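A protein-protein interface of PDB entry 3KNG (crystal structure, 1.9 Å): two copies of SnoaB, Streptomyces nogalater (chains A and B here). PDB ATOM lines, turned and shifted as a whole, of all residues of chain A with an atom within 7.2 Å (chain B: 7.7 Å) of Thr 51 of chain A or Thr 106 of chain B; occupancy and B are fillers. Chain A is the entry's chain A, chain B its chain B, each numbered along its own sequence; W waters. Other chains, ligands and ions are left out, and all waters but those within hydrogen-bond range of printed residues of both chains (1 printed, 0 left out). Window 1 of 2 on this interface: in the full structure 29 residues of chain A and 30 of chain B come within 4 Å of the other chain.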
ATOM      1  N   PHE A  34      -2.625  -7.001  -2.842  1.00  0.00           N
ATOM      2  CA  PHE A  34      -3.754  -7.612  -2.143  1.00  0.00           C
ATOM      3  C   PHE A  34      -3.396  -7.970  -0.704  1.00  0.00           C
ATOM      4  O   PHE A  34      -4.187  -7.728   0.210  1.00  0.00           O
ATOM      5  CB  PHE A  34      -4.303  -8.850  -2.860  1.00  0.00           C
ATOM      6  CG  PHE A  34      -5.544  -9.401  -2.213  1.00  0.00           C
ATOM      7  CD1 PHE A  34      -6.800  -8.958  -2.613  1.00  0.00           C
ATOM      8  CD2 PHE A  34      -5.459 -10.324  -1.172  1.00  0.00           C
ATOM      9  CE1 PHE A  34      -7.953  -9.444  -2.004  1.00  0.00           C
ATOM     10  CE2 PHE A  34      -6.605 -10.814  -0.556  1.00  0.00           C
ATOM     11  CZ  PHE A  34      -7.853 -10.372  -0.974  1.00  0.00           C
ATOM     12  N   PHE A  47     -13.193  -8.550  12.034  1.00  0.00           N
ATOM     13  CA  PHE A  47     -12.626  -9.415  10.995  1.00  0.00           C
ATOM     14  C   PHE A  47     -12.502 -10.838  11.527  1.00  0.00           C
ATOM     15  O   PHE A  47     -11.975 -11.047  12.623  1.00  0.00           O
ATOM     16  CB  PHE A  47     -11.262  -8.909  10.507  1.00  0.00           C
ATOM     17  CG  PHE A  47     -10.599  -9.825   9.506  1.00  0.00           C
ATOM     18  CD1 PHE A  47     -10.938  -9.766   8.157  1.00  0.00           C
ATOM     19  CD2 PHE A  47      -9.648 -10.759   9.917  1.00  0.00           C
ATOM     20  CE1 PHE A  47     -10.335 -10.616   7.230  1.00  0.00           C
ATOM     21  CE2 PHE A  47      -9.040 -11.612   8.997  1.00  0.00           C
ATOM     22  CZ  PHE A  47      -9.383 -11.539   7.651  1.00  0.00           C
ATOM     23  N   ARG A  49     -11.940 -14.032   9.098  1.00  0.00           N
ATOM     24  CA  ARG A  49     -10.981 -14.740   8.252  1.00  0.00           C
ATOM     25  C   ARG A  49     -11.186 -14.361   6.789  1.00  0.00           C
ATOM     26  O   ARG A  49     -12.237 -13.834   6.421  1.00  0.00           O
ATOM     27  CB  ARG A  49     -11.120 -16.261   8.423  1.00  0.00           C
ATOM     28  CG  ARG A  49     -12.443 -16.821   7.922  1.00  0.00           C
ATOM     29  CD  ARG A  49     -12.546 -18.323   8.100  1.00  0.00           C
ATOM     30  NE  ARG A  49     -13.870 -18.798   7.705  1.00  0.00           N
ATOM     31  CZ  ARG A  49     -14.925 -18.855   8.514  1.00  0.00           C
ATOM     32  NH1 ARG A  49     -14.826 -18.478   9.783  1.00  0.00           N
ATOM     33  NH2 ARG A  49     -16.087 -19.296   8.053  1.00  0.00           N
ATOM     34  N   HIS A  50     -10.178 -14.622   5.961  1.00  0.00           N
ATOM     35  CA  HIS A  50     -10.332 -14.521   4.513  1.00  0.00           C
ATOM     36  C   HIS A  50      -9.497 -15.590   3.825  1.00  0.00           C
ATOM     37  O   HIS A  50      -8.538 -16.097   4.397  1.00  0.00           O
ATOM     38  CB  HIS A  50      -9.932 -13.131   3.995  1.00  0.00           C
ATOM     39  CG  HIS A  50      -8.509 -13.046   3.530  1.00  0.00           C
ATOM     40  ND1 HIS A  50      -8.132 -13.286   2.225  1.00  0.00           N
ATOM     41  CD2 HIS A  50      -7.370 -12.766   4.205  1.00  0.00           C
ATOM     42  CE1 HIS A  50      -6.822 -13.151   2.116  1.00  0.00           C
ATOM     43  NE2 HIS A  50      -6.336 -12.837   3.303  1.00  0.00           N
ATOM     44  N   THR A  51      -9.874 -15.921   2.594  1.00  0.00           N
ATOM     45  CA  THR A  51      -9.047 -16.748   1.725  1.00  0.00           C
ATOM     46  C   THR A  51      -9.031 -16.151   0.318  1.00  0.00           C
ATOM     47  O   THR A  51     -10.088 -15.942  -0.284  1.00  0.00           O
ATOM     48  CB  THR A  51      -9.553 -18.210   1.673  1.00  0.00           C
ATOM     49  OG1 THR A  51      -9.633 -18.740   3.002  1.00  0.00           O
ATOM     50  CG2 THR A  51      -8.621 -19.083   0.837  1.00  0.00           C
ATOM     51  N   LEU A  52      -7.836 -15.860  -0.192  1.00  0.00           N
ATOM     52  CA  LEU A  52      -7.679 -15.478  -1.592  1.00  0.00           C
ATOM     53  C   LEU A  52      -7.442 -16.732  -2.425  1.00  0.00           C
ATOM     54  O   LEU A  52      -6.521 -17.506  -2.153  1.00  0.00           O
ATOM     55  CB  LEU A  52      -6.532 -14.478  -1.783  1.00  0.00           C
ATOM     56  CG  LEU A  52      -6.267 -13.992  -3.218  1.00  0.00           C
ATOM     57  CD1 LEU A  52      -7.336 -13.010  -3.689  1.00  0.00           C
ATOM     58  CD2 LEU A  52      -4.886 -13.365  -3.322  1.00  0.00           C
ATOM     59  N   LEU A  53      -8.285 -16.923  -3.436  1.00  0.00           N
ATOM     60  CA  LEU A  53      -8.231 -18.095  -4.308  1.00  0.00           C
ATOM     61  C   LEU A  53      -7.831 -17.685  -5.727  1.00  0.00           C
ATOM     62  O   LEU A  53      -8.253 -16.631  -6.200  1.00  0.00           O
ATOM     63  CB  LEU A  53      -9.601 -18.787  -4.343  1.00  0.00           C
ATOM     64  CG  LEU A  53     -10.280 -19.251  -3.047  1.00  0.00           C
ATOM     65  CD1 LEU A  53     -11.770 -19.465  -3.268  1.00  0.00           C
ATOM     66  CD2 LEU A  53      -9.629 -20.517  -2.501  1.00  0.00           C
ATOM     67  N   VAL A  63     -10.634 -15.113  -6.679  1.00  0.00           N
ATOM     68  CA  VAL A  63     -11.810 -14.867  -5.843  1.00  0.00           C
ATOM     69  C   VAL A  63     -11.377 -14.733  -4.386  1.00  0.00           C
ATOM     70  O   VAL A  63     -10.619 -15.564  -3.880  1.00  0.00           O
ATOM     71  CB  VAL A  63     -12.885 -15.987  -5.987  1.00  0.00           C
ATOM     72  CG1 VAL A  63     -13.933 -15.900  -4.877  1.00  0.00           C
ATOM     73  CG2 VAL A  63     -13.564 -15.914  -7.347  1.00  0.00           C
ATOM     74  N   ASN A  64     -11.848 -13.684  -3.721  1.00  0.00           N
ATOM     75  CA  ASN A  64     -11.626 -13.539  -2.291  1.00  0.00           C
ATOM     76  C   ASN A  64     -12.905 -13.766  -1.500  1.00  0.00           C
ATOM     77  O   ASN A  64     -13.970 -13.255  -1.858  1.00  0.00           O
ATOM     78  CB  ASN A  64     -11.042 -12.167  -1.955  1.00  0.00           C
ATOM     79  CG  ASN A  64     -10.648 -12.042  -0.493  1.00  0.00           C
ATOM     80  OD1 ASN A  64      -9.870 -12.845   0.026  1.00  0.00           O
ATOM     81  ND2 ASN A  64     -11.176 -11.025   0.176  1.00  0.00           N
ATOM     82  N   ILE A  65     -12.779 -14.543  -0.430  1.00  0.00           N
ATOM     83  CA  ILE A  65     -13.887 -14.797   0.482  1.00  0.00           C
ATOM     84  C   ILE A  65     -13.483 -14.281   1.857  1.00  0.00           C
ATOM     85  O   ILE A  65     -12.488 -14.725   2.431  1.00  0.00           O
ATOM     86  CB  ILE A  65     -14.238 -16.308   0.559  1.00  0.00           C
ATOM     87  CG1 ILE A  65     -14.511 -16.887  -0.834  1.00  0.00           C
ATOM     88  CG2 ILE A  65     -15.437 -16.547   1.466  1.00  0.00           C
ATOM     89  CD1 ILE A  65     -14.645 -18.390  -0.855  1.00  0.00           C
ATOM     90  N   ALA A  66     -14.247 -13.326   2.382  1.00  0.00           N
ATOM     91  CA  ALA A  66     -13.925 -12.735   3.685  1.00  0.00           C
ATOM     92  C   ALA A  66     -15.116 -12.743   4.637  1.00  0.00           C
ATOM     93  O   ALA A  66     -16.219 -12.341   4.263  1.00  0.00           O
ATOM     94  CB  ALA A  66     -13.383 -11.320   3.512  1.00  0.00           C
ATOM     95  N   VAL A  67     -14.884 -13.198   5.867  1.00  0.00           N
ATOM     96  CA  VAL A  67     -15.947 -13.308   6.866  1.00  0.00           C
ATOM     97  C   VAL A  67     -15.802 -12.240   7.955  1.00  0.00           C
ATOM     98  O   VAL A  67     -14.705 -11.983   8.454  1.00  0.00           O
ATOM     99  CB  VAL A  67     -16.014 -14.733   7.489  1.00  0.00           C
ATOM    100  CG1 VAL A  67     -17.199 -14.863   8.443  1.00  0.00           C
ATOM    101  CG2 VAL A  67     -16.110 -15.795   6.398  1.00  0.00           C
ATOM    102  N   GLU B  14      -5.348 -29.236  -2.214  1.00  0.00           N
ATOM    103  CA  GLU B  14      -6.741 -28.883  -1.965  1.00  0.00           C
ATOM    104  C   GLU B  14      -7.285 -27.932  -3.032  1.00  0.00           C
ATOM    105  O   GLU B  14      -6.611 -26.976  -3.420  1.00  0.00           O
ATOM    106  CB  GLU B  14      -6.831 -28.249  -0.576  1.00  0.00           C
ATOM    107  CG  GLU B  14      -8.215 -27.879  -0.095  1.00  0.00           C
ATOM    108  CD  GLU B  14      -8.196 -27.325   1.317  1.00  0.00           C
ATOM    109  OE1 GLU B  14      -8.431 -26.110   1.484  1.00  0.00           O
ATOM    110  OE2 GLU B  14      -7.938 -28.102   2.261  1.00  0.00           O
ATOM    111  N   THR B  16     -10.874 -25.659  -4.380  1.00  0.00           N
ATOM    112  CA  THR B  16     -12.133 -25.066  -3.968  1.00  0.00           C
ATOM    113  C   THR B  16     -12.971 -24.784  -5.205  1.00  0.00           C
ATOM    114  O   THR B  16     -12.534 -24.069  -6.109  1.00  0.00           O
ATOM    115  CB  THR B  16     -11.898 -23.762  -3.182  1.00  0.00           C
ATOM    116  OG1 THR B  16     -11.111 -24.037  -2.017  1.00  0.00           O
ATOM    117  CG2 THR B  16     -13.213 -23.145  -2.756  1.00  0.00           C
ATOM    118  N   ARG B  49     -15.537 -29.635   3.012  1.00  0.00           N
ATOM    119  CA  ARG B  49     -16.605 -28.806   3.570  1.00  0.00           C
ATOM    120  C   ARG B  49     -17.327 -28.038   2.470  1.00  0.00           C
ATOM    121  O   ARG B  49     -16.837 -27.954   1.341  1.00  0.00           O
ATOM    122  CB  ARG B  49     -16.054 -27.832   4.627  1.00  0.00           C
ATOM    123  CG  ARG B  49     -15.064 -26.807   4.090  1.00  0.00           C
ATOM    124  CD  ARG B  49     -14.465 -25.955   5.197  1.00  0.00           C
ATOM    125  NE  ARG B  49     -13.473 -25.022   4.663  1.00  0.00           N
ATOM    126  CZ  ARG B  49     -12.171 -25.276   4.558  1.00  0.00           C
ATOM    127  NH1 ARG B  49     -11.675 -26.443   4.955  1.00  0.00           N
ATOM    128  NH2 ARG B  49     -11.358 -24.358   4.054  1.00  0.00           N
ATOM    129  N   THR B 102      -7.418 -22.727  -6.412  1.00  0.00           N
ATOM    130  CA  THR B 102      -6.490 -23.134  -5.362  1.00  0.00           C
ATOM    131  C   THR B 102      -6.207 -21.939  -4.466  1.00  0.00           C
ATOM    132  O   THR B 102      -6.242 -20.788  -4.908  1.00  0.00           O
ATOM    133  CB  THR B 102      -5.165 -23.696  -5.912  1.00  0.00           C
ATOM    134  OG1 THR B 102      -4.573 -22.747  -6.808  1.00  0.00           O
ATOM    135  CG2 THR B 102      -5.393 -25.014  -6.645  1.00  0.00           C
ATOM    136  N   ALA B 103      -5.955 -22.217  -3.189  1.00  0.00           N
ATOM    137  CA  ALA B 103      -5.702 -21.166  -2.205  1.00  0.00           C
ATOM    138  C   ALA B 103      -4.319 -20.538  -2.374  1.00  0.00           C
ATOM    139  O   ALA B 103      -3.322 -21.242  -2.559  1.00  0.00           O
ATOM    140  CB  ALA B 103      -5.877 -21.704  -0.792  1.00  0.00           C
ATOM    141  N   ARG B 104      -4.277 -19.209  -2.307  1.00  0.00           N
ATOM    142  CA  ARG B 104      -3.028 -18.453  -2.401  1.00  0.00           C
ATOM    143  C   ARG B 104      -2.662 -17.792  -1.070  1.00  0.00           C
ATOM    144  O   ARG B 104      -1.498 -17.813  -0.665  1.00  0.00           O
ATOM    145  CB  ARG B 104      -3.113 -17.396  -3.509  1.00  0.00           C
ATOM    146  CG  ARG B 104      -3.301 -17.956  -4.917  1.00  0.00           C
ATOM    147  CD  ARG B 104      -2.085 -18.742  -5.403  1.00  0.00           C
ATOM    148  NE  ARG B 104      -0.912 -17.887  -5.578  1.00  0.00           N
ATOM    149  CZ  ARG B 104       0.347 -18.312  -5.524  1.00  0.00           C
ATOM    150  NH1 ARG B 104       0.620 -19.591  -5.292  1.00  0.00           N
ATOM    151  NH2 ARG B 104       1.340 -17.451  -5.697  1.00  0.00           N
ATOM    152  N   GLN B 105      -3.658 -17.210  -0.402  1.00  0.00           N
ATOM    153  CA  GLN B 105      -3.465 -16.522   0.881  1.00  0.00           C
ATOM    154  C   GLN B 105      -4.637 -16.772   1.828  1.00  0.00           C
ATOM    155  O   GLN B 105      -5.784 -16.861   1.383  1.00  0.00           O
ATOM    156  CB  GLN B 105      -3.346 -15.007   0.675  1.00  0.00           C
ATOM    157  CG  GLN B 105      -2.170 -14.527  -0.166  1.00  0.00           C
ATOM    158  CD  GLN B 105      -2.225 -13.031  -0.457  1.00  0.00           C
ATOM    159  OE1 GLN B 105      -2.880 -12.267   0.254  1.00  0.00           O
ATOM    160  NE2 GLN B 105      -1.529 -12.610  -1.507  1.00  0.00           N
ATOM    161  N   THR B 106      -4.339 -16.883   3.124  1.00  0.00           N
ATOM    162  CA  THR B 106      -5.358 -17.000   4.178  1.00  0.00           C
ATOM    163  C   THR B 106      -4.941 -16.211   5.411  1.00  0.00           C
ATOM    164  O   THR B 106      -3.763 -16.213   5.781  1.00  0.00           O
ATOM    165  CB  THR B 106      -5.588 -18.464   4.648  1.00  0.00           C
ATOM    166  OG1 THR B 106      -4.331 -19.094   4.925  1.00  0.00           O
ATOM    167  CG2 THR B 106      -6.339 -19.273   3.609  1.00  0.00           C
ATOM    168  N   LEU B 107      -5.904 -15.553   6.047  1.00  0.00           N
ATOM    169  CA  LEU B 107      -5.714 -14.945   7.360  1.00  0.00           C
ATOM    170  C   LEU B 107      -6.906 -15.365   8.221  1.00  0.00           C
ATOM    171  O   LEU B 107      -8.019 -15.457   7.706  1.00  0.00           O
ATOM    172  CB  LEU B 107      -5.623 -13.418   7.268  1.00  0.00           C
ATOM    173  CG  LEU B 107      -4.414 -12.790   6.561  1.00  0.00           C
ATOM    174  CD1 LEU B 107      -4.617 -11.294   6.385  1.00  0.00           C
ATOM    175  CD2 LEU B 107      -3.107 -13.070   7.300  1.00  0.00           C
ATOM    176  N   PRO B 108      -6.686 -15.648   9.523  1.00  0.00           N
ATOM    177  CA  PRO B 108      -5.411 -15.645  10.243  1.00  0.00           C
ATOM    178  C   PRO B 108      -4.481 -16.758   9.767  1.00  0.00           C
ATOM    179  O   PRO B 108      -4.941 -17.779   9.247  1.00  0.00           O
ATOM    180  CB  PRO B 108      -5.827 -15.866  11.700  1.00  0.00           C
ATOM    181  CG  PRO B 108      -7.120 -16.581  11.616  1.00  0.00           C
ATOM    182  CD  PRO B 108      -7.805 -16.016  10.410  1.00  0.00           C
ATOM    183  N   GLU B 109      -3.182 -16.545   9.952  1.00  0.00           N
ATOM    184  CA  GLU B 109      -2.155 -17.348   9.297  1.00  0.00           C
ATOM    185  C   GLU B 109      -1.458 -18.279  10.281  1.00  0.00           C
ATOM    186  O   GLU B 109      -2.106 -19.068  10.967  1.00  0.00           O
ATOM    187  CB  GLU B 109      -1.130 -16.428   8.622  1.00  0.00           C
ATOM    188  CG  GLU B 109      -0.245 -17.113   7.592  1.00  0.00           C
HETATM  189  O   HOH W   1      -3.545 -12.221   2.915  1.00  0.00           O
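O of Leu 107 of chain B lies within hydrogen-bond range of N of His 50 of chain A, 2.9 Å away.
The backbone carbonyl oxygen (O) of Leu 52 of chain A lies within hydrogen-bond range of the backbone NH (N) of Arg 104 of chain B, 2.8 Å away.
The backbone NH of Leu 52 of chain A sits at hydrogen-bond distance from the backbone carbonyl oxygen of Gln 105 of chain B, at 2.8 Å.
O of Arg 49 of chain A lies within hydrogen-bond range of N of Val 67 of chain A, 2.8 Å away.
ND1 of His 50 of chain A sits at hydrogen-bond distance from OD1 of Asn 64 of chain A (2.8 Å).
O of Thr 51 of chain A lies close to OD1 of Asn 64 of chain A (3.1 Å).
The backbone NH of Thr 51 of chain A sits at hydrogen-bond distance from the backbone carbonyl oxygen of Ile 65 of chain A (2.9 Å).
The backbone carbonyl oxygen (O) of Val 63 of chain A is in hydrogen-bond range of the backbone NH (N) of Leu 53 of chain A (2.7 Å).
Among the printed residues, merely in contact across the chains: Arg 49 of chain A with Leu 107 of chain B (3.1 Å), Thr 51 of chain A with Gln 105 of chain B (3.3 Å), His 50 of chain A with Thr 106 of chain B (3.3 Å), Thr 51 of chain A with Thr 106 of chain B (3.4 Å), Leu 53 of chain A with Thr 102 of chain B (3.4 Å), Phe 34 of chain A with Gln 105 of chain B (3.5 Å), Leu 52 of chain A with Ala 103 of chain B (3.8 Å), Leu 53 of chain A with Thr 16 of chain B (3.8 Å), Arg 49 of chain A with Pro 108 of chain B (3.9 Å), His 50 of chain A with Gln 105 of chain B (3.9 Å) and Leu 53 of chain A with Ala 103 of chain B (3.99 Å).
Printed residues of chain B within 4 Å of Thr 51 of chain A: Gln 105 and Thr 106.
Printed residues of chain B within 4 Å of Leu 53 of chain A: Thr 16 (3.8 Å), Thr 102 (3.4 Å) and Ala 103 (3.99 Å).
Printed residues of chain A within 4 Å of Thr 16 of chain B: Leu 53.
Printed residues of chain A within 4 Å of Ala 103 of chain B: Leu 52 (3.8 Å) and Leu 53 (3.99 Å).
Printed residues of chain A within 4 Å of Thr 106 of chain B: His 50 and Thr 51.
Printed residues of chain A within 4 Å of Leu 107 of chain B: Arg 49 (3.1 Å) and His 50 (2.9 Å).
The nearest printed residue of chain A that does not touch Thr 106 of chain B is Leu 52 of chain A (4.9 Å).
The nearest printed residue of chain A that does not touch Leu 107 of chain B is Phe 47 of chain A (4.1 Å).
Of the 12 printed residues of chain A, 6 touch a printed residue of chain B.
Of the 11 printed residues of chain B, 8 touch a printed residue of chain A.
1 position is printed for both chains.
Water W1 lies within hydrogen-bond range of OE1 of Gln 105 of chain B and NE2 of His 50 of chain A.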
